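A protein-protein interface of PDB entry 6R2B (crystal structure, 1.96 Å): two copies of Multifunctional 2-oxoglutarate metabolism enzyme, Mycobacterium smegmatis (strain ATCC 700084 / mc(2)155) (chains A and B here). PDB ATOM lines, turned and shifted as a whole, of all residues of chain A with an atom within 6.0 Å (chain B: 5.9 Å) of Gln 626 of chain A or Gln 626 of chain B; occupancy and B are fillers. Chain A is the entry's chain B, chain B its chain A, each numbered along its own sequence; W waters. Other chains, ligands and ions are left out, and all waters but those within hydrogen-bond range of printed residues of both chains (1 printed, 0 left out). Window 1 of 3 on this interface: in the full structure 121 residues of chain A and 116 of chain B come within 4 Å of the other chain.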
ATOM      1  N   VAL A 622      -0.183  -1.839 -20.432  1.00  0.00           N
ATOM      2  CA  VAL A 622       0.336  -0.604 -21.047  1.00  0.00           C
ATOM      3  C   VAL A 622      -0.369   0.652 -20.473  1.00  0.00           C
ATOM      4  O   VAL A 622       0.186   1.744 -20.575  1.00  0.00           O
ATOM      5  CB  VAL A 622       0.318  -0.655 -22.607  1.00  0.00           C
ATOM      6  CG1 VAL A 622      -1.075  -0.390 -23.184  1.00  0.00           C
ATOM      7  CG2 VAL A 622       1.353   0.313 -23.199  1.00  0.00           C
ATOM      8  N   ASN A 623      -1.520   0.490 -19.779  1.00  0.00           N
ATOM      9  CA  ASN A 623      -2.160   1.650 -19.124  1.00  0.00           C
ATOM     10  C   ASN A 623      -1.268   2.220 -17.987  1.00  0.00           C
ATOM     11  O   ASN A 623      -1.464   3.356 -17.584  1.00  0.00           O
ATOM     12  CB  ASN A 623      -3.575   1.329 -18.601  1.00  0.00           C
ATOM     13  CG  ASN A 623      -3.697   0.112 -17.730  1.00  0.00           C
ATOM     14  OD1 ASN A 623      -2.735  -0.608 -17.481  1.00  0.00           O
ATOM     15  ND2 ASN A 623      -4.905  -0.155 -17.258  1.00  0.00           N
ATOM     16  N   GLY A 624      -0.264   1.456 -17.541  1.00  0.00           N
ATOM     17  CA  GLY A 624       0.731   1.905 -16.565  1.00  0.00           C
ATOM     18  C   GLY A 624       1.642   2.973 -17.174  1.00  0.00           C
ATOM     19  O   GLY A 624       2.273   3.740 -16.444  1.00  0.00           O
ATOM     20  N   ALA A 625       1.685   3.053 -18.526  1.00  0.00           N
ATOM     21  CA  ALA A 625       2.462   4.057 -19.258  1.00  0.00           C
ATOM     22  C   ALA A 625       1.532   5.089 -19.929  1.00  0.00           C
ATOM     23  O   ALA A 625       1.912   5.697 -20.933  1.00  0.00           O
ATOM     24  CB  ALA A 625       3.315   3.376 -20.310  1.00  0.00           C
ATOM     25  N   GLN A 626       0.315   5.284 -19.385  1.00  0.00           N
ATOM     26  CA  GLN A 626      -0.666   6.172 -20.026  1.00  0.00           C
ATOM     27  C   GLN A 626      -0.143   7.589 -20.241  1.00  0.00           C
ATOM     28  O   GLN A 626      -0.390   8.155 -21.304  1.00  0.00           O
ATOM     29  CB  GLN A 626      -1.990   6.221 -19.265  1.00  0.00           C
ATOM     30  CG  GLN A 626      -3.154   6.747 -20.153  1.00  0.00           C
ATOM     31  CD  GLN A 626      -3.472   5.755 -21.254  1.00  0.00           C
ATOM     32  OE1 GLN A 626      -3.792   4.604 -20.982  1.00  0.00           O
ATOM     33  NE2 GLN A 626      -3.366   6.162 -22.516  1.00  0.00           N
ATOM     34  N   SER A 627       0.591   8.152 -19.257  1.00  0.00           N
ATOM     35  CA  SER A 627       1.147   9.500 -19.382  1.00  0.00           C
ATOM     36  C   SER A 627       2.077   9.600 -20.592  1.00  0.00           C
ATOM     37  O   SER A 627       2.029  10.587 -21.291  1.00  0.00           O
ATOM     38  CB  SER A 627       1.905   9.899 -18.118  1.00  0.00           C
ATOM     39  OG  SER A 627       1.046   9.946 -16.996  1.00  0.00           O
ATOM     40  N   ILE A 628       2.900   8.569 -20.849  1.00  0.00           N
ATOM     41  CA  ILE A 628       3.807   8.566 -22.011  1.00  0.00           C
ATOM     42  C   ILE A 628       2.995   8.482 -23.323  1.00  0.00           C
ATOM     43  O   ILE A 628       3.281   9.223 -24.259  1.00  0.00           O
ATOM     44  CB  ILE A 628       4.879   7.439 -21.913  1.00  0.00           C
ATOM     45  CG1 ILE A 628       5.741   7.593 -20.616  1.00  0.00           C
ATOM     46  CG2 ILE A 628       5.760   7.379 -23.191  1.00  0.00           C
ATOM     47  CD1 ILE A 628       6.596   8.974 -20.522  1.00  0.00           C
ATOM     48  N   ILE A 629       1.999   7.600 -23.391  1.00  0.00           N
ATOM     49  CA  ILE A 629       1.164   7.434 -24.601  1.00  0.00           C
ATOM     50  C   ILE A 629       0.424   8.754 -24.905  1.00  0.00           C
ATOM     51  O   ILE A 629       0.467   9.252 -26.028  1.00  0.00           O
ATOM     52  CB  ILE A 629       0.172   6.249 -24.386  1.00  0.00           C
ATOM     53  CG1 ILE A 629       0.935   4.900 -24.351  1.00  0.00           C
ATOM     54  CG2 ILE A 629      -0.940   6.229 -25.479  1.00  0.00           C
ATOM     55  CD1 ILE A 629       0.124   3.766 -23.683  1.00  0.00           C
ATOM     56  N   ASP A 630      -0.240   9.318 -23.895  1.00  0.00           N
ATOM     57  CA  ASP A 630      -0.992  10.569 -24.033  1.00  0.00           C
ATOM     58  C   ASP A 630      -0.141  11.804 -24.328  1.00  0.00           C
ATOM     59  O   ASP A 630      -0.515  12.617 -25.174  1.00  0.00           O
ATOM     60  CB  ASP A 630      -1.769  10.849 -22.741  1.00  0.00           C
ATOM     61  CG  ASP A 630      -2.896   9.887 -22.460  1.00  0.00           C
ATOM     62  OD1 ASP A 630      -3.109   8.963 -23.276  1.00  0.00           O
ATOM     63  OD2 ASP A 630      -3.566  10.054 -21.427  1.00  0.00           O
ATOM     64  N   GLU A 631       0.953  11.976 -23.584  1.00  0.00           N
ATOM     65  CA  GLU A 631       1.742  13.201 -23.640  1.00  0.00           C
ATOM     66  C   GLU A 631       2.904  13.180 -24.611  1.00  0.00           C
ATOM     67  O   GLU A 631       3.375  14.248 -24.966  1.00  0.00           O
ATOM     68  CB  GLU A 631       2.282  13.541 -22.239  1.00  0.00           C
ATOM     69  CG  GLU A 631       1.197  13.662 -21.176  1.00  0.00           C
ATOM     70  CD  GLU A 631       0.169  14.732 -21.471  1.00  0.00           C
ATOM     71  OE1 GLU A 631       0.575  15.843 -21.883  1.00  0.00           O
ATOM     72  OE2 GLU A 631      -1.037  14.467 -21.272  1.00  0.00           O
ATOM     73  N   ARG A 668      -8.965   2.832 -26.979  1.00  0.00           N
ATOM     74  CA  ARG A 668      -8.276   3.992 -26.423  1.00  0.00           C
ATOM     75  C   ARG A 668      -7.257   4.549 -27.414  1.00  0.00           C
ATOM     76  O   ARG A 668      -7.180   5.765 -27.583  1.00  0.00           O
ATOM     77  CB  ARG A 668      -7.599   3.648 -25.095  1.00  0.00           C
ATOM     78  CG  ARG A 668      -7.060   4.898 -24.378  1.00  0.00           C
ATOM     79  CD  ARG A 668      -6.628   4.552 -22.965  1.00  0.00           C
ATOM     80  NE  ARG A 668      -7.779   4.204 -22.130  1.00  0.00           N
ATOM     81  CZ  ARG A 668      -7.685   3.674 -20.921  1.00  0.00           C
ATOM     82  NH1 ARG A 668      -6.495   3.391 -20.403  1.00  0.00           N
ATOM     83  NH2 ARG A 668      -8.777   3.414 -20.222  1.00  0.00           N
ATOM     84  N   LEU A 672      -7.330   8.202 -29.341  1.00  0.00           N
ATOM     85  CA  LEU A 672      -6.173   9.107 -29.318  1.00  0.00           C
ATOM     86  C   LEU A 672      -5.731   9.488 -30.727  1.00  0.00           C
ATOM     87  O   LEU A 672      -5.199  10.585 -30.923  1.00  0.00           O
ATOM     88  CB  LEU A 672      -5.004   8.458 -28.560  1.00  0.00           C
ATOM     89  CG  LEU A 672      -5.126   8.472 -27.024  1.00  0.00           C
ATOM     90  CD1 LEU A 672      -4.208   7.455 -26.407  1.00  0.00           C
ATOM     91  CD2 LEU A 672      -4.867   9.874 -26.453  1.00  0.00           C
ATOM     92  N   VAL B 622      -4.969  13.573 -14.435  1.00  0.00           N
ATOM     93  CA  VAL B 622      -5.564  12.335 -13.892  1.00  0.00           C
ATOM     94  C   VAL B 622      -5.120  11.088 -14.702  1.00  0.00           C
ATOM     95  O   VAL B 622      -5.208   9.964 -14.181  1.00  0.00           O
ATOM     96  CB  VAL B 622      -7.107  12.427 -13.728  1.00  0.00           C
ATOM     97  CG1 VAL B 622      -7.845  12.220 -15.048  1.00  0.00           C
ATOM     98  CG2 VAL B 622      -7.610  11.449 -12.667  1.00  0.00           C
ATOM     99  N   ASN B 623      -4.551  11.277 -15.911  1.00  0.00           N
ATOM    100  CA  ASN B 623      -4.041  10.134 -16.679  1.00  0.00           C
ATOM    101  C   ASN B 623      -2.839   9.486 -15.964  1.00  0.00           C
ATOM    102  O   ASN B 623      -2.524   8.349 -16.266  1.00  0.00           O
ATOM    103  CB  ASN B 623      -3.706  10.512 -18.137  1.00  0.00           C
ATOM    104  CG  ASN B 623      -2.771  11.674 -18.315  1.00  0.00           C
ATOM    105  OD1 ASN B 623      -2.347  12.336 -17.355  1.00  0.00           O
ATOM    106  ND2 ASN B 623      -2.446  11.958 -19.572  1.00  0.00           N
ATOM    107  N   GLY B 624      -2.237  10.185 -14.989  1.00  0.00           N
ATOM    108  CA  GLY B 624      -1.172   9.647 -14.132  1.00  0.00           C
ATOM    109  C   GLY B 624      -1.710   8.568 -13.198  1.00  0.00           C
ATOM    110  O   GLY B 624      -0.952   7.753 -12.676  1.00  0.00           O
ATOM    111  N   ALA B 625      -3.041   8.538 -12.997  1.00  0.00           N
ATOM    112  CA  ALA B 625      -3.724   7.536 -12.174  1.00  0.00           C
ATOM    113  C   ALA B 625      -4.548   6.562 -13.048  1.00  0.00           C
ATOM    114  O   ALA B 625      -5.524   5.984 -12.564  1.00  0.00           O
ATOM    115  CB  ALA B 625      -4.641   8.228 -11.181  1.00  0.00           C
ATOM    116  N   GLN B 626      -4.173   6.393 -14.329  1.00  0.00           N
ATOM    117  CA  GLN B 626      -4.953   5.579 -15.258  1.00  0.00           C
ATOM    118  C   GLN B 626      -5.152   4.142 -14.769  1.00  0.00           C
ATOM    119  O   GLN B 626      -6.259   3.618 -14.912  1.00  0.00           O
ATOM    120  CB  GLN B 626      -4.349   5.565 -16.670  1.00  0.00           C
ATOM    121  CG  GLN B 626      -5.377   5.108 -17.729  1.00  0.00           C
ATOM    122  CD  GLN B 626      -6.473   6.139 -17.879  1.00  0.00           C
ATOM    123  OE1 GLN B 626      -6.212   7.291 -18.193  1.00  0.00           O
ATOM    124  NE2 GLN B 626      -7.716   5.754 -17.657  1.00  0.00           N
ATOM    125  N   SER B 627      -4.112   3.526 -14.166  1.00  0.00           N
ATOM    126  CA  SER B 627      -4.218   2.161 -13.646  1.00  0.00           C
ATOM    127  C   SER B 627      -5.311   2.062 -12.583  1.00  0.00           C
ATOM    128  O   SER B 627      -6.048   1.093 -12.582  1.00  0.00           O
ATOM    129  CB  SER B 627      -2.892   1.697 -13.060  1.00  0.00           C
ATOM    130  OG  SER B 627      -1.895   1.649 -14.058  1.00  0.00           O
ATOM    131  N   ILE B 628      -5.448   3.080 -11.709  1.00  0.00           N
ATOM    132  CA  ILE B 628      -6.489   3.074 -10.665  1.00  0.00           C
ATOM    133  C   ILE B 628      -7.874   3.235 -11.323  1.00  0.00           C
ATOM    134  O   ILE B 628      -8.800   2.525 -10.955  1.00  0.00           O
ATOM    135  CB  ILE B 628      -6.224   4.159  -9.572  1.00  0.00           C
ATOM    136  CG1 ILE B 628      -4.852   3.914  -8.860  1.00  0.00           C
ATOM    137  CG2 ILE B 628      -7.401   4.222  -8.544  1.00  0.00           C
ATOM    138  CD1 ILE B 628      -4.713   2.501  -8.090  1.00  0.00           C
ATOM    139  N   ILE B 629      -8.008   4.168 -12.275  1.00  0.00           N
ATOM    140  CA  ILE B 629      -9.272   4.423 -12.984  1.00  0.00           C
ATOM    141  C   ILE B 629      -9.725   3.125 -13.694  1.00  0.00           C
ATOM    142  O   ILE B 629     -10.858   2.657 -13.495  1.00  0.00           O
ATOM    143  CB  ILE B 629      -9.096   5.620 -13.978  1.00  0.00           C
ATOM    144  CG1 ILE B 629      -8.870   6.958 -13.214  1.00  0.00           C
ATOM    145  CG2 ILE B 629     -10.290   5.730 -14.963  1.00  0.00           C
ATOM    146  CD1 ILE B 629      -8.288   8.095 -14.121  1.00  0.00           C
ATOM    147  N   ASP B 630      -8.827   2.542 -14.491  1.00  0.00           N
ATOM    148  CA  ASP B 630      -9.109   1.321 -15.265  1.00  0.00           C
ATOM    149  C   ASP B 630      -9.346   0.075 -14.430  1.00  0.00           C
ATOM    150  O   ASP B 630     -10.261  -0.706 -14.728  1.00  0.00           O
ATOM    151  CB  ASP B 630      -7.938   1.016 -16.208  1.00  0.00           C
ATOM    152  CG  ASP B 630      -7.726   2.010 -17.324  1.00  0.00           C
ATOM    153  OD1 ASP B 630      -8.533   2.960 -17.438  1.00  0.00           O
ATOM    154  OD2 ASP B 630      -6.745   1.844 -18.090  1.00  0.00           O
ATOM    155  N   GLU B 631      -8.489  -0.158 -13.436  1.00  0.00           N
ATOM    156  CA  GLU B 631      -8.499  -1.415 -12.678  1.00  0.00           C
ATOM    157  C   GLU B 631      -9.329  -1.410 -11.417  1.00  0.00           C
ATOM    158  O   GLU B 631      -9.677  -2.489 -10.956  1.00  0.00           O
ATOM    159  CB  GLU B 631      -7.070  -1.816 -12.320  1.00  0.00           C
ATOM    160  CG  GLU B 631      -6.157  -1.939 -13.532  1.00  0.00           C
ATOM    161  CD  GLU B 631      -6.605  -2.968 -14.548  1.00  0.00           C
ATOM    162  OE1 GLU B 631      -7.008  -4.077 -14.125  1.00  0.00           O
ATOM    163  OE2 GLU B 631      -6.531  -2.677 -15.763  1.00  0.00           O
ATOM    164  N   ARG B 668     -12.621   9.501 -22.604  1.00  0.00           N
ATOM    165  CA  ARG B 668     -12.033   8.291 -22.026  1.00  0.00           C
ATOM    166  C   ARG B 668     -12.928   7.721 -20.929  1.00  0.00           C
ATOM    167  O   ARG B 668     -13.138   6.506 -20.881  1.00  0.00           O
ATOM    168  CB  ARG B 668     -10.622   8.554 -21.494  1.00  0.00           C
ATOM    169  CG  ARG B 668      -9.901   7.249 -21.097  1.00  0.00           C
ATOM    170  CD  ARG B 668      -8.434   7.515 -20.811  1.00  0.00           C
ATOM    171  NE  ARG B 668      -7.703   7.868 -22.032  1.00  0.00           N
ATOM    172  CZ  ARG B 668      -6.472   8.359 -22.034  1.00  0.00           C
ATOM    173  NH1 ARG B 668      -5.850   8.609 -20.891  1.00  0.00           N
ATOM    174  NH2 ARG B 668      -5.858   8.617 -23.177  1.00  0.00           N
ATOM    175  N   LEU B 672     -14.972   4.122 -20.903  1.00  0.00           N
ATOM    176  CA  LEU B 672     -14.853   3.190 -19.786  1.00  0.00           C
ATOM    177  C   LEU B 672     -16.217   2.851 -19.190  1.00  0.00           C
ATOM    178  O   LEU B 672     -16.398   1.748 -18.677  1.00  0.00           O
ATOM    179  CB  LEU B 672     -13.941   3.769 -18.686  1.00  0.00           C
ATOM    180  CG  LEU B 672     -12.442   3.710 -18.977  1.00  0.00           C
ATOM    181  CD1 LEU B 672     -11.702   4.657 -18.095  1.00  0.00           C
ATOM    182  CD2 LEU B 672     -11.898   2.282 -18.818  1.00  0.00           C
HETATM  183  O   HOH W   1      -0.884   5.757 -15.985  1.00  0.00           O
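Water W1 bridges the backbone carbonyl oxygen of Asn 623 of chain A (2.9 Å) and the backbone carbonyl oxygen of Asn 623 of chain B (3.1 Å).
Asn 623 of chain A touches Glu 631 of chain B, and with the chains exchanged Glu 631 of chain A touches Asn 623 of chain B. Gln 626 of chain A touches its own counterpart, Gln 626 of chain B. Gln 626 of chain A touches Arg 668 of chain B, and with the chains exchanged Arg 668 of chain A touches Gln 626 of chain B. Asp 630 of chain A touches Arg 668 of chain B, and with the chains exchanged Arg 668 of chain A touches Asp 630 of chain B. Positions printed for both chains: 622, 623, 624, 625, 626, 627, 628, 629, 630, 631, 668 and 672. Of the 18 pairs that touch across the chains among the printed residues, 18 have their exchanged pair printed and touching as well.
The side-chain amide nitrogen of Asn 623 of chain B lies within hydrogen-bond range of the side-chain carboxylate of Asp 630 of chain A, 2.9 Å away. ND2 of Asn 623 of chain B sits at hydrogen-bond distance from OE2 of Glu 631 of chain A (3.3 Å). The side-chain carboxylate (OD2) of Asp 630 of chain B is in hydrogen-bond range of the side-chain amide nitrogen (ND2) of Asn 623 of chain A (2.8 Å). NH1 of Arg 668 of chain A is in salt-bridge range of OD2 of Asp 630 of chain B, at 2.8 Å. The side-chain amide nitrogen (ND2) of Asn 623 of chain A sits at hydrogen-bond distance from the side-chain carboxylate (OE2) of Glu 631 of chain B (3.4 Å). OD2 of Asp 630 of chain A lies within salt-bridge range of NH1 of Arg 668 of chain B (2.8 Å).
Gln 626 of chain A touches just these residues of chain B: Asn 623, Gln 626 and Arg 668. Of chain A, only Asn 623 (3.7 Å), Gln 626 (3.6 Å) and Arg 668 (3.4 Å) come within 4 Å of Gln 626 of chain B. Of the printed residues of chain B, Ser 627 of chain A touches Asn 623 and Gly 624. Printed residues of chain B within 4 Å of Leu 672 of chain A: Arg 668. Val 622 of chain A touches none of the printed residues of chain B. Val 622 of chain B touches none of the printed residues of chain A. The nearest residue of chain A that does not touch Gln 626 of chain B is Asp 630 of chain A (5.0 Å). The nearest printed residue of chain B that does not touch Leu 672 of chain A is Asn 623 of chain B (7.6 Å).
NE2 of Gln 626 of chain B lies within hydrogen-bond range of OD1 of Asp 630 of chain B, 2.9 Å away. The guanidinium group (NH1) of Arg 668 of chain B sits at hydrogen-bond distance from the side-chain amide oxygen (OE1) of Gln 626 of chain B (3.0 Å). The side-chain carboxylate (OD1) of Asp 630 of chain A sits at hydrogen-bond distance from the side-chain amide nitrogen (NE2) of Gln 626 of chain A (2.9 Å). The guanidinium group of Arg 668 of chain A is in hydrogen-bond range of the side-chain amide oxygen of Gln 626 of chain A.
Of the 12 printed residues of chain B, 8 touch a printed residue of chain A. Hydrophobic or aromatic side chains of chain B within 4 Å of the printed part of chain A: Leu 672. Of the 12 printed residues of chain A, 8 touch a printed residue of chain B. Printed residues of chain A that touch a printed residue of chain B: Asn 623, Gly 624, Gln 626, Ser 627, Asp 630, Glu 631, Arg 668 and Leu 672. Hydrophobic or aromatic side chains of chain A that line the printed part of chain B: Leu 672.
Among the printed residues, merely in contact across the chains: Asn 623 of chain A with Gln 626 of chain B (3.7 Å), Asn 623 of chain A with Ser 627 of chain B (3.9 Å), Gly 624 of chain A with Ser 627 of chain B (3.6 Å), Gln 626 of chain A with Asn 623 of chain B (3.7 Å), Gln 626 of chain A with Gln 626 of chain B (3.6 Å), Gln 626 of chain A with Arg 668 of chain B (3.4 Å), Ser 627 of chain A with Asn 623 of chain B (3.98 Å), Ser 627 of chain A with Gly 624 of chain B (3.6 Å), Arg 668 of chain A with Gln 626 of chain B (3.4 Å), Arg 668 of chain A with Arg 668 of chain B (3.6 Å), Arg 668 of chain A with Leu 672 of chain B (3.6 Å) and Leu 672 of chain A with Arg 668 of chain B (3.6 Å).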
